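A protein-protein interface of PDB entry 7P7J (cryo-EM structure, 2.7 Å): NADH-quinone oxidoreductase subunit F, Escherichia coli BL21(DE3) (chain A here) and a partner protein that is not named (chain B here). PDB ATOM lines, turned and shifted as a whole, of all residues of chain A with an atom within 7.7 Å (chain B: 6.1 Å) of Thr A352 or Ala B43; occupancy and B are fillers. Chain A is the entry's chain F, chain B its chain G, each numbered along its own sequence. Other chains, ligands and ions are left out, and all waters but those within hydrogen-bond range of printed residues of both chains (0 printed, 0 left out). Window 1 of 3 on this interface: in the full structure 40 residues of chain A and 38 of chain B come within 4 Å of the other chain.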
ATOM      1  N   SER A 347      11.236   3.996 -12.863  1.00  0.00           N
ATOM      2  CA  SER A 347      10.277   2.907 -12.928  1.00  0.00           C
ATOM      3  C   SER A 347       9.728   2.624 -11.537  1.00  0.00           C
ATOM      4  O   SER A 347      10.389   2.859 -10.525  1.00  0.00           O
ATOM      5  CB  SER A 347      10.941   1.656 -13.497  1.00  0.00           C
ATOM      6  OG  SER A 347      10.047   0.561 -13.524  1.00  0.00           O
ATOM      7  N   GLY A 349       8.616  -0.480 -10.798  1.00  0.00           N
ATOM      8  CA  GLY A 349       8.939  -1.865 -10.538  1.00  0.00           C
ATOM      9  C   GLY A 349       7.773  -2.818 -10.522  1.00  0.00           C
ATOM     10  O   GLY A 349       7.953  -3.976 -10.135  1.00  0.00           O
ATOM     11  N   TRP A 350       6.580  -2.372 -10.917  1.00  0.00           N
ATOM     12  CA  TRP A 350       5.411  -3.241 -10.854  1.00  0.00           C
ATOM     13  C   TRP A 350       5.450  -4.305 -11.937  1.00  0.00           C
ATOM     14  O   TRP A 350       5.181  -5.481 -11.672  1.00  0.00           O
ATOM     15  CB  TRP A 350       4.132  -2.420 -10.978  1.00  0.00           C
ATOM     16  CG  TRP A 350       2.902  -3.244 -10.991  1.00  0.00           C
ATOM     17  CD1 TRP A 350       2.073  -3.465 -12.047  1.00  0.00           C
ATOM     18  CD2 TRP A 350       2.352  -3.967  -9.890  1.00  0.00           C
ATOM     19  NE1 TRP A 350       1.039  -4.282 -11.672  1.00  0.00           N
ATOM     20  CE2 TRP A 350       1.188  -4.602 -10.349  1.00  0.00           C
ATOM     21  CE3 TRP A 350       2.733  -4.138  -8.557  1.00  0.00           C
ATOM     22  CZ2 TRP A 350       0.402  -5.396  -9.526  1.00  0.00           C
ATOM     23  CZ3 TRP A 350       1.951  -4.925  -7.743  1.00  0.00           C
ATOM     24  CH2 TRP A 350       0.799  -5.544  -8.229  1.00  0.00           C
ATOM     25  N   CYS A 351       5.776  -3.919 -13.164  1.00  0.00           N
ATOM     26  CA  CYS A 351       5.577  -4.806 -14.293  1.00  0.00           C
ATOM     27  C   CYS A 351       6.885  -5.084 -15.018  1.00  0.00           C
ATOM     28  O   CYS A 351       7.777  -4.237 -15.084  1.00  0.00           O
ATOM     29  CB  CYS A 351       4.502  -4.253 -15.242  1.00  0.00           C
ATOM     30  SG  CYS A 351       4.970  -3.004 -16.415  1.00  0.00           S
ATOM     31  N   THR A 352       6.975  -6.307 -15.543  1.00  0.00           N
ATOM     32  CA  THR A 352       8.243  -6.869 -16.010  1.00  0.00           C
ATOM     33  C   THR A 352       8.914  -6.120 -17.161  1.00  0.00           C
ATOM     34  O   THR A 352      10.131  -5.889 -17.062  1.00  0.00           O
ATOM     35  CB  THR A 352       8.038  -8.347 -16.366  1.00  0.00           C
ATOM     36  OG1 THR A 352       7.579  -9.056 -15.211  1.00  0.00           O
ATOM     37  CG2 THR A 352       9.327  -8.983 -16.852  1.00  0.00           C
ATOM     38  N   PRO A 353       8.237  -5.746 -18.269  1.00  0.00           N
ATOM     39  CA  PRO A 353       8.995  -5.184 -19.403  1.00  0.00           C
ATOM     40  C   PRO A 353       9.709  -3.886 -19.091  1.00  0.00           C
ATOM     41  O   PRO A 353      10.892  -3.769 -19.406  1.00  0.00           O
ATOM     42  CB  PRO A 353       7.921  -4.991 -20.482  1.00  0.00           C
ATOM     43  CG  PRO A 353       6.850  -5.898 -20.110  1.00  0.00           C
ATOM     44  CD  PRO A 353       6.812  -5.831 -18.632  1.00  0.00           C
ATOM     45  N   CYS A 354       9.052  -2.941 -18.423  1.00  0.00           N
ATOM     46  CA  CYS A 354       9.722  -1.711 -18.014  1.00  0.00           C
ATOM     47  C   CYS A 354      10.845  -2.004 -17.026  1.00  0.00           C
ATOM     48  O   CYS A 354      12.011  -1.691 -17.300  1.00  0.00           O
ATOM     49  CB  CYS A 354       8.682  -0.756 -17.437  1.00  0.00           C
ATOM     50  SG  CYS A 354       9.162   0.678 -16.447  1.00  0.00           S
ATOM     51  N   ARG A 355      10.526  -2.743 -15.955  1.00  0.00           N
ATOM     52  CA  ARG A 355      11.443  -2.963 -14.835  1.00  0.00           C
ATOM     53  C   ARG A 355      12.706  -3.708 -15.255  1.00  0.00           C
ATOM     54  O   ARG A 355      13.800  -3.406 -14.767  1.00  0.00           O
ATOM     55  CB  ARG A 355      10.717  -3.727 -13.723  1.00  0.00           C
ATOM     56  CG  ARG A 355      11.625  -4.380 -12.688  1.00  0.00           C
ATOM     57  CD  ARG A 355      10.888  -5.301 -11.742  1.00  0.00           C
ATOM     58  NE  ARG A 355      10.673  -6.619 -12.325  1.00  0.00           N
ATOM     59  CZ  ARG A 355       9.481  -7.140 -12.568  1.00  0.00           C
ATOM     60  NH1 ARG A 355       8.371  -6.494 -12.258  1.00  0.00           N
ATOM     61  NH2 ARG A 355       9.399  -8.341 -13.128  1.00  0.00           N
ATOM     62  N   ASP A 356      12.584  -4.681 -16.153  1.00  0.00           N
ATOM     63  CA  ASP A 356      13.721  -5.494 -16.551  1.00  0.00           C
ATOM     64  C   ASP A 356      14.180  -5.260 -17.982  1.00  0.00           C
ATOM     65  O   ASP A 356      15.114  -5.931 -18.426  1.00  0.00           O
ATOM     66  CB  ASP A 356      13.402  -6.979 -16.356  1.00  0.00           C
ATOM     67  CG  ASP A 356      13.427  -7.393 -14.904  1.00  0.00           C
ATOM     68  OD1 ASP A 356      14.199  -6.797 -14.128  1.00  0.00           O
ATOM     69  OD2 ASP A 356      12.680  -8.319 -14.536  1.00  0.00           O
ATOM     70  N   GLY A 357      13.585  -4.319 -18.710  1.00  0.00           N
ATOM     71  CA  GLY A 357      14.006  -4.076 -20.067  1.00  0.00           C
ATOM     72  C   GLY A 357      14.535  -2.677 -20.265  1.00  0.00           C
ATOM     73  O   GLY A 357      15.368  -2.460 -21.147  1.00  0.00           O
ATOM     74  N   LEU A 358      14.060  -1.710 -19.478  1.00  0.00           N
ATOM     75  CA  LEU A 358      14.723  -0.412 -19.467  1.00  0.00           C
ATOM     76  C   LEU A 358      16.162  -0.474 -18.950  1.00  0.00           C
ATOM     77  O   LEU A 358      17.017   0.190 -19.557  1.00  0.00           O
ATOM     78  CB  LEU A 358      13.874   0.603 -18.691  1.00  0.00           C
ATOM     79  CG  LEU A 358      12.599   1.064 -19.394  1.00  0.00           C
ATOM     80  CD1 LEU A 358      11.952   2.204 -18.633  1.00  0.00           C
ATOM     81  CD2 LEU A 358      12.889   1.475 -20.824  1.00  0.00           C
ATOM     82  N   PRO A 359      16.508  -1.201 -17.871  1.00  0.00           N
ATOM     83  CA  PRO A 359      17.937  -1.328 -17.529  1.00  0.00           C
ATOM     84  C   PRO A 359      18.776  -2.037 -18.577  1.00  0.00           C
ATOM     85  O   PRO A 359      19.962  -1.712 -18.715  1.00  0.00           O
ATOM     86  CB  PRO A 359      17.909  -2.112 -16.211  1.00  0.00           C
ATOM     87  CG  PRO A 359      16.618  -1.786 -15.628  1.00  0.00           C
ATOM     88  CD  PRO A 359      15.683  -1.754 -16.780  1.00  0.00           C
ATOM     89  N   LEU A 388       7.677  -2.772 -25.641  1.00  0.00           N
ATOM     90  CA  LEU A 388       7.331  -1.942 -24.495  1.00  0.00           C
ATOM     91  C   LEU A 388       6.310  -0.882 -24.885  1.00  0.00           C
ATOM     92  O   LEU A 388       6.263   0.194 -24.290  1.00  0.00           O
ATOM     93  CB  LEU A 388       8.571  -1.286 -23.894  1.00  0.00           C
ATOM     94  CG  LEU A 388       9.245  -1.955 -22.699  1.00  0.00           C
ATOM     95  CD1 LEU A 388      10.087  -3.134 -23.144  1.00  0.00           C
ATOM     96  CD2 LEU A 388      10.096  -0.947 -21.960  1.00  0.00           C
ATOM     97  N   LYS A 392       1.420  -3.623 -23.766  1.00  0.00           N
ATOM     98  CA  LYS A 392       2.424  -4.592 -23.341  1.00  0.00           C
ATOM     99  C   LYS A 392       2.835  -4.368 -21.892  1.00  0.00           C
ATOM    100  O   LYS A 392       3.024  -5.330 -21.140  1.00  0.00           O
ATOM    101  CB  LYS A 392       3.640  -4.525 -24.261  1.00  0.00           C
ATOM    102  CG  LYS A 392       3.496  -5.331 -25.539  1.00  0.00           C
ATOM    103  CD  LYS A 392       3.002  -4.472 -26.680  1.00  0.00           C
ATOM    104  CE  LYS A 392       3.122  -5.197 -28.001  1.00  0.00           C
ATOM    105  NZ  LYS A 392       2.678  -4.339 -29.130  1.00  0.00           N
ATOM    106  N   THR A 393       2.981  -3.113 -21.484  1.00  0.00           N
ATOM    107  CA  THR A 393       3.311  -2.767 -20.111  1.00  0.00           C
ATOM    108  C   THR A 393       2.056  -2.356 -19.352  1.00  0.00           C
ATOM    109  O   THR A 393       0.987  -2.148 -19.928  1.00  0.00           O
ATOM    110  CB  THR A 393       4.352  -1.647 -20.072  1.00  0.00           C
ATOM    111  OG1 THR A 393       3.854  -0.505 -20.776  1.00  0.00           O
ATOM    112  CG2 THR A 393       5.636  -2.109 -20.717  1.00  0.00           C
ATOM    113  N   PHE A 394       2.200  -2.246 -18.034  1.00  0.00           N
ATOM    114  CA  PHE A 394       1.045  -2.003 -17.177  1.00  0.00           C
ATOM    115  C   PHE A 394       0.561  -0.562 -17.265  1.00  0.00           C
ATOM    116  O   PHE A 394      -0.648  -0.312 -17.229  1.00  0.00           O
ATOM    117  CB  PHE A 394       1.384  -2.365 -15.736  1.00  0.00           C
ATOM    118  CG  PHE A 394       0.192  -2.455 -14.842  1.00  0.00           C
ATOM    119  CD1 PHE A 394      -0.641  -3.555 -14.891  1.00  0.00           C
ATOM    120  CD2 PHE A 394      -0.098  -1.441 -13.950  1.00  0.00           C
ATOM    121  CE1 PHE A 394      -1.738  -3.643 -14.071  1.00  0.00           C
ATOM    122  CE2 PHE A 394      -1.194  -1.526 -13.127  1.00  0.00           C
ATOM    123  CZ  PHE A 394      -2.012  -2.628 -13.185  1.00  0.00           C
ATOM    124  N   CYS B  33       2.303 -13.944 -12.128  1.00  0.00           N
ATOM    125  CA  CYS B  33       1.755 -13.137 -11.048  1.00  0.00           C
ATOM    126  C   CYS B  33       0.328 -13.509 -10.670  1.00  0.00           C
ATOM    127  O   CYS B  33      -0.139 -13.083  -9.610  1.00  0.00           O
ATOM    128  CB  CYS B  33       1.823 -11.653 -11.416  1.00  0.00           C
ATOM    129  SG  CYS B  33       0.558 -11.083 -12.559  1.00  0.00           S
ATOM    130  N   VAL B  41      -3.610  -9.232 -11.078  1.00  0.00           N
ATOM    131  CA  VAL B  41      -3.113  -7.876 -10.877  1.00  0.00           C
ATOM    132  C   VAL B  41      -2.352  -7.401 -12.106  1.00  0.00           C
ATOM    133  O   VAL B  41      -2.056  -6.210 -12.238  1.00  0.00           O
ATOM    134  CB  VAL B  41      -2.231  -7.789  -9.623  1.00  0.00           C
ATOM    135  CG1 VAL B  41      -3.098  -7.630  -8.400  1.00  0.00           C
ATOM    136  CG2 VAL B  41      -1.343  -9.010  -9.514  1.00  0.00           C
ATOM    137  N   GLY B  42      -2.031  -8.322 -13.007  1.00  0.00           N
ATOM    138  CA  GLY B  42      -1.385  -7.969 -14.259  1.00  0.00           C
ATOM    139  C   GLY B  42       0.029  -7.441 -14.151  1.00  0.00           C
ATOM    140  O   GLY B  42       0.416  -6.560 -14.927  1.00  0.00           O
ATOM    141  N   ALA B  43       0.824  -7.977 -13.226  1.00  0.00           N
ATOM    142  CA  ALA B  43       2.173  -7.461 -13.020  1.00  0.00           C
ATOM    143  C   ALA B  43       3.181  -8.097 -13.975  1.00  0.00           C
ATOM    144  O   ALA B  43       3.834  -7.399 -14.752  1.00  0.00           O
ATOM    145  CB  ALA B  43       2.599  -7.679 -11.568  1.00  0.00           C
ATOM    146  N   CYS B  44       3.309  -9.422 -13.946  1.00  0.00           N
ATOM    147  CA  CYS B  44       4.431 -10.083 -14.606  1.00  0.00           C
ATOM    148  C   CYS B  44       4.378 -10.013 -16.130  1.00  0.00           C
ATOM    149  O   CYS B  44       5.410 -10.236 -16.769  1.00  0.00           O
ATOM    150  CB  CYS B  44       4.500 -11.543 -14.174  1.00  0.00           C
ATOM    151  SG  CYS B  44       3.138 -12.523 -14.797  1.00  0.00           S
ATOM    152  N   ARG B  45       3.209  -9.735 -16.716  1.00  0.00           N
ATOM    153  CA  ARG B  45       3.010  -9.611 -18.170  1.00  0.00           C
ATOM    154  C   ARG B  45       3.389 -10.882 -18.928  1.00  0.00           C
ATOM    155  O   ARG B  45       3.742 -10.831 -20.106  1.00  0.00           O
ATOM    156  CB  ARG B  45       3.748  -8.399 -18.750  1.00  0.00           C
ATOM    157  CG  ARG B  45       3.506  -7.088 -18.011  1.00  0.00           C
ATOM    158  CD  ARG B  45       2.040  -6.773 -17.835  1.00  0.00           C
ATOM    159  NE  ARG B  45       1.488  -6.016 -18.947  1.00  0.00           N
ATOM    160  CZ  ARG B  45       0.277  -5.476 -18.948  1.00  0.00           C
ATOM    161  NH1 ARG B  45      -0.524  -5.584 -17.902  1.00  0.00           N
ATOM    162  NH2 ARG B  45      -0.140  -4.818 -20.024  1.00  0.00           N
ATOM    163  N   GLN B  46       3.292 -12.035 -18.269  1.00  0.00           N
ATOM    164  CA  GLN B  46       3.657 -13.311 -18.866  1.00  0.00           C
ATOM    165  C   GLN B  46       2.503 -13.976 -19.605  1.00  0.00           C
ATOM    166  O   GLN B  46       2.742 -14.774 -20.514  1.00  0.00           O
ATOM    167  CB  GLN B  46       4.188 -14.252 -17.776  1.00  0.00           C
ATOM    168  CG  GLN B  46       4.799 -15.557 -18.255  1.00  0.00           C
ATOM    169  CD  GLN B  46       6.017 -15.348 -19.114  1.00  0.00           C
ATOM    170  OE1 GLN B  46       7.096 -15.062 -18.612  1.00  0.00           O
ATOM    171  NE2 GLN B  46       5.850 -15.480 -20.420  1.00  0.00           N
ATOM    172  N   CYS B  66      -4.902 -12.829 -17.965  1.00  0.00           N
ATOM    173  CA  CYS B  66      -5.365 -12.828 -16.583  1.00  0.00           C
ATOM    174  C   CYS B  66      -6.224 -11.609 -16.283  1.00  0.00           C
ATOM    175  O   CYS B  66      -7.084 -11.664 -15.401  1.00  0.00           O
ATOM    176  CB  CYS B  66      -4.177 -12.903 -15.627  1.00  0.00           C
ATOM    177  SG  CYS B  66      -3.292 -11.362 -15.370  1.00  0.00           S
ATOM    178  N   SER B  89      10.151 -13.018 -24.578  1.00  0.00           N
ATOM    179  CA  SER B  89      10.885 -11.828 -24.162  1.00  0.00           C
ATOM    180  C   SER B  89      10.685 -11.533 -22.684  1.00  0.00           C
ATOM    181  O   SER B  89      11.612 -11.077 -22.012  1.00  0.00           O
ATOM    182  CB  SER B  89      10.463 -10.632 -25.004  1.00  0.00           C
ATOM    183  OG  SER B  89      10.847 -10.816 -26.350  1.00  0.00           O
ATOM    184  N   VAL B  90       9.479 -11.768 -22.165  1.00  0.00           N
ATOM    185  CA  VAL B  90       9.231 -11.570 -20.739  1.00  0.00           C
ATOM    186  C   VAL B  90      10.055 -12.553 -19.915  1.00  0.00           C
ATOM    187  O   VAL B  90      10.679 -12.176 -18.913  1.00  0.00           O
ATOM    188  CB  VAL B  90       7.725 -11.683 -20.436  1.00  0.00           C
ATOM    189  CG1 VAL B  90       7.477 -11.773 -18.939  1.00  0.00           C
ATOM    190  CG2 VAL B  90       6.982 -10.499 -21.013  1.00  0.00           C
ATOM    191  N   VAL B  91      10.097 -13.819 -20.344  1.00  0.00           N
ATOM    192  CA  VAL B  91      10.922 -14.815 -19.656  1.00  0.00           C
ATOM    193  C   VAL B  91      12.401 -14.438 -19.735  1.00  0.00           C
ATOM    194  O   VAL B  91      13.146 -14.581 -18.756  1.00  0.00           O
ATOM    195  CB  VAL B  91      10.638 -16.222 -20.225  1.00  0.00           C
ATOM    196  CG1 VAL B  91      11.902 -17.053 -20.376  1.00  0.00           C
ATOM    197  CG2 VAL B  91       9.666 -16.952 -19.333  1.00  0.00           C
ATOM    198  N   TRP B  93      13.654 -11.340 -20.032  1.00  0.00           N
ATOM    199  CA  TRP B  93      13.874 -10.197 -19.150  1.00  0.00           C
ATOM    200  C   TRP B  93      13.934 -10.628 -17.696  1.00  0.00           C
ATOM    201  O   TRP B  93      14.691 -10.058 -16.904  1.00  0.00           O
ATOM    202  CB  TRP B  93      12.772  -9.158 -19.333  1.00  0.00           C
ATOM    203  CG  TRP B  93      12.849  -8.405 -20.608  1.00  0.00           C
ATOM    204  CD1 TRP B  93      13.973  -7.970 -21.236  1.00  0.00           C
ATOM    205  CD2 TRP B  93      11.749  -7.990 -21.416  1.00  0.00           C
ATOM    206  NE1 TRP B  93      13.642  -7.312 -22.392  1.00  0.00           N
ATOM    207  CE2 TRP B  93      12.280  -7.309 -22.523  1.00  0.00           C
ATOM    208  CE3 TRP B  93      10.365  -8.127 -21.310  1.00  0.00           C
ATOM    209  CZ2 TRP B  93      11.477  -6.772 -23.520  1.00  0.00           C
ATOM    210  CZ3 TRP B  93       9.572  -7.599 -22.300  1.00  0.00           C
ATOM    211  CH2 TRP B  93      10.127  -6.925 -23.388  1.00  0.00           C
ATOM    212  N   LEU B  94      13.115 -11.611 -17.318  1.00  0.00           N
ATOM    213  CA  LEU B  94      13.240 -12.188 -15.986  1.00  0.00           C
ATOM    214  C   LEU B  94      14.571 -12.902 -15.817  1.00  0.00           C
ATOM    215  O   LEU B  94      15.132 -12.920 -14.718  1.00  0.00           O
ATOM    216  CB  LEU B  94      12.090 -13.155 -15.716  1.00  0.00           C
ATOM    217  CG  LEU B  94      10.707 -12.521 -15.621  1.00  0.00           C
ATOM    218  CD1 LEU B  94       9.656 -13.583 -15.415  1.00  0.00           C
ATOM    219  CD2 LEU B  94      10.670 -11.499 -14.507  1.00  0.00           C
ATOM    220  N   ILE B 151      11.612 -12.724  -9.070  1.00  0.00           N
ATOM    221  CA  ILE B 151      11.220 -12.207 -10.369  1.00  0.00           C
ATOM    222  C   ILE B 151      10.232 -11.060 -10.243  1.00  0.00           C
ATOM    223  O   ILE B 151       9.701 -10.598 -11.252  1.00  0.00           O
ATOM    224  CB  ILE B 151      10.647 -13.322 -11.264  1.00  0.00           C
ATOM    225  CG1 ILE B 151       9.385 -13.897 -10.631  1.00  0.00           C
ATOM    226  CG2 ILE B 151      11.686 -14.398 -11.510  1.00  0.00           C
ATOM    227  CD1 ILE B 151       8.764 -14.998 -11.414  1.00  0.00           C
ATOM    228  N   ALA B 152       9.981 -10.597  -9.013  1.00  0.00           N
ATOM    229  CA  ALA B 152       9.075  -9.488  -8.708  1.00  0.00           C
ATOM    230  C   ALA B 152       7.674  -9.739  -9.263  1.00  0.00           C
ATOM    231  O   ALA B 152       7.112  -8.925  -9.994  1.00  0.00           O
ATOM    232  CB  ALA B 152       9.637  -8.154  -9.202  1.00  0.00           C
ATOM    233  N   CYS B 153       7.122 -10.895  -8.921  1.00  0.00           N
ATOM    234  CA  CYS B 153       5.779 -11.262  -9.332  1.00  0.00           C
ATOM    235  C   CYS B 153       4.717 -10.871  -8.315  1.00  0.00           C
ATOM    236  O   CYS B 153       3.525 -11.012  -8.609  1.00  0.00           O
ATOM    237  CB  CYS B 153       5.717 -12.766  -9.591  1.00  0.00           C
ATOM    238  SG  CYS B 153       5.421 -13.747  -8.126  1.00  0.00           S
ATOM    239  N   TYR B 154       5.125 -10.412  -7.130  1.00  0.00           N
ATOM    240  CA  TYR B 154       4.265  -9.861  -6.080  1.00  0.00           C
ATOM    241  C   TYR B 154       3.265 -10.870  -5.524  1.00  0.00           C
ATOM    242  O   TYR B 154       2.281 -10.476  -4.901  1.00  0.00           O
ATOM    243  CB  TYR B 154       3.524  -8.606  -6.561  1.00  0.00           C
ATOM    244  CG  TYR B 154       4.428  -7.425  -6.807  1.00  0.00           C
ATOM    245  CD1 TYR B 154       5.067  -7.260  -8.027  1.00  0.00           C
ATOM    246  CD2 TYR B 154       4.643  -6.474  -5.824  1.00  0.00           C
ATOM    247  CE1 TYR B 154       5.898  -6.190  -8.257  1.00  0.00           C
ATOM    248  CE2 TYR B 154       5.469  -5.397  -6.048  1.00  0.00           C
ATOM    249  CZ  TYR B 154       6.093  -5.261  -7.267  1.00  0.00           C
ATOM    250  OH  TYR B 154       6.921  -4.192  -7.502  1.00  0.00           O
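Of the 16 printed residues of chain A, 11 touch a printed residue of chain B. Hydrophobic or aromatic side chains of chain B that line the printed part of chain A: Val B41, Ala B43, Val B90, Trp B93, Leu B94, Ala B152 and Tyr B154. Among the printed residues, 22 pairs touch across the chains. Among the printed residues, no Asp or Glu carboxylate lies within 4 Å of a Lys or Arg side-chain nitrogen of the other chain.
The backbone NH (N) of Gly A349 is in hydrogen-bond range of the side-chain hydroxyl (OG) of Ser A347. The side-chain hydroxyl (OG1) of Thr A352 is in hydrogen-bond range of the guanidinium group (NH2) of Arg A355 (2.9 Å). The side-chain carboxylate (OD2) of Asp A356 is in salt-bridge range of the guanidinium group (NE) of Arg A355, at 3.4 Å. SG of Cys B33 sits close to N of Ala B43 (3.2 Å). The guanidinium group of Arg B45 lies within hydrogen-bond range of the backbone carbonyl oxygen of Gly B42, 3.3 Å away. N of Gln B46 sits close to SG of Cys B44 (3.5 Å).
The backbone carbonyl oxygen of Gly A349 is in hydrogen-bond range of the side-chain hydroxyl of Tyr B154, 2.8 Å away. The backbone NH (N) of Thr A352 is in hydrogen-bond range of the backbone carbonyl oxygen (O) of Ala B43 (3.4 Å). The side-chain hydroxyl of Thr A352 sits at hydrogen-bond distance from the backbone carbonyl oxygen of Cys B44 (2.9 Å). O of Ile B151 lies within hydrogen-bond range of NH2 of Arg A355 (3.0 Å). O of Lys A392 is in hydrogen-bond range of NE of Arg B45, at 2.8 Å. The backbone carbonyl oxygen (O) of Thr A393 is in hydrogen-bond range of the guanidinium group (NH2) of Arg B45 (2.9 Å).
Thr A352 touches just these residues of chain B: Ala B43, Cys B44, Val B90 and Leu B94. Of chain A, only Trp A350, Cys A351 and Thr A352 come within 4 Å of Ala B43. Of chain A, only Phe A394 comes within 4 Å of Gly B42. Of the printed residues of chain B, Phe A394 touches Val B41, Gly B42 and Arg B45. Printed residues of chain A within 4 Å of Leu B94: Thr A352, Arg A355 and Asp A356. Printed residues of chain B within 4 Å of Leu A388: Trp B93 (3.8 Å). Of the printed residues of chain B, Trp A350 touches Val B41, Ala B43 and Tyr B154. The nearest residue of chain B that does not touch Thr A352 is Trp B93 (4.2 Å).
Among the printed residues, pairs that only touch across the chains: Cys A351 with Ala B43 (3.2 Å), Phe A394 with Val B41 (3.2 Å), Phe A394 with Gly B42 (3.2 Å), Asp A356 with Trp B93 (3.4 Å), Trp A350 with Ala B43 (3.4 Å), Arg A355 with Ala B152 (3.5 Å), Trp A350 with Val B41 (3.6 Å), Trp A350 with Tyr B154 (3.6 Å), Pro A353 with Trp B93 (3.6 Å), Pro A353 with Arg B45 (3.6 Å), Phe A394 with Arg B45 (3.6 Å), Arg A355 with Leu B94 (3.7 Å), Thr A352 with Leu B94 (3.7 Å), Asp A356 with Leu B94 (3.8 Å), Leu A388 with Trp B93 (3.8 Å) and Thr A352 with Val B90 (3.9 Å).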
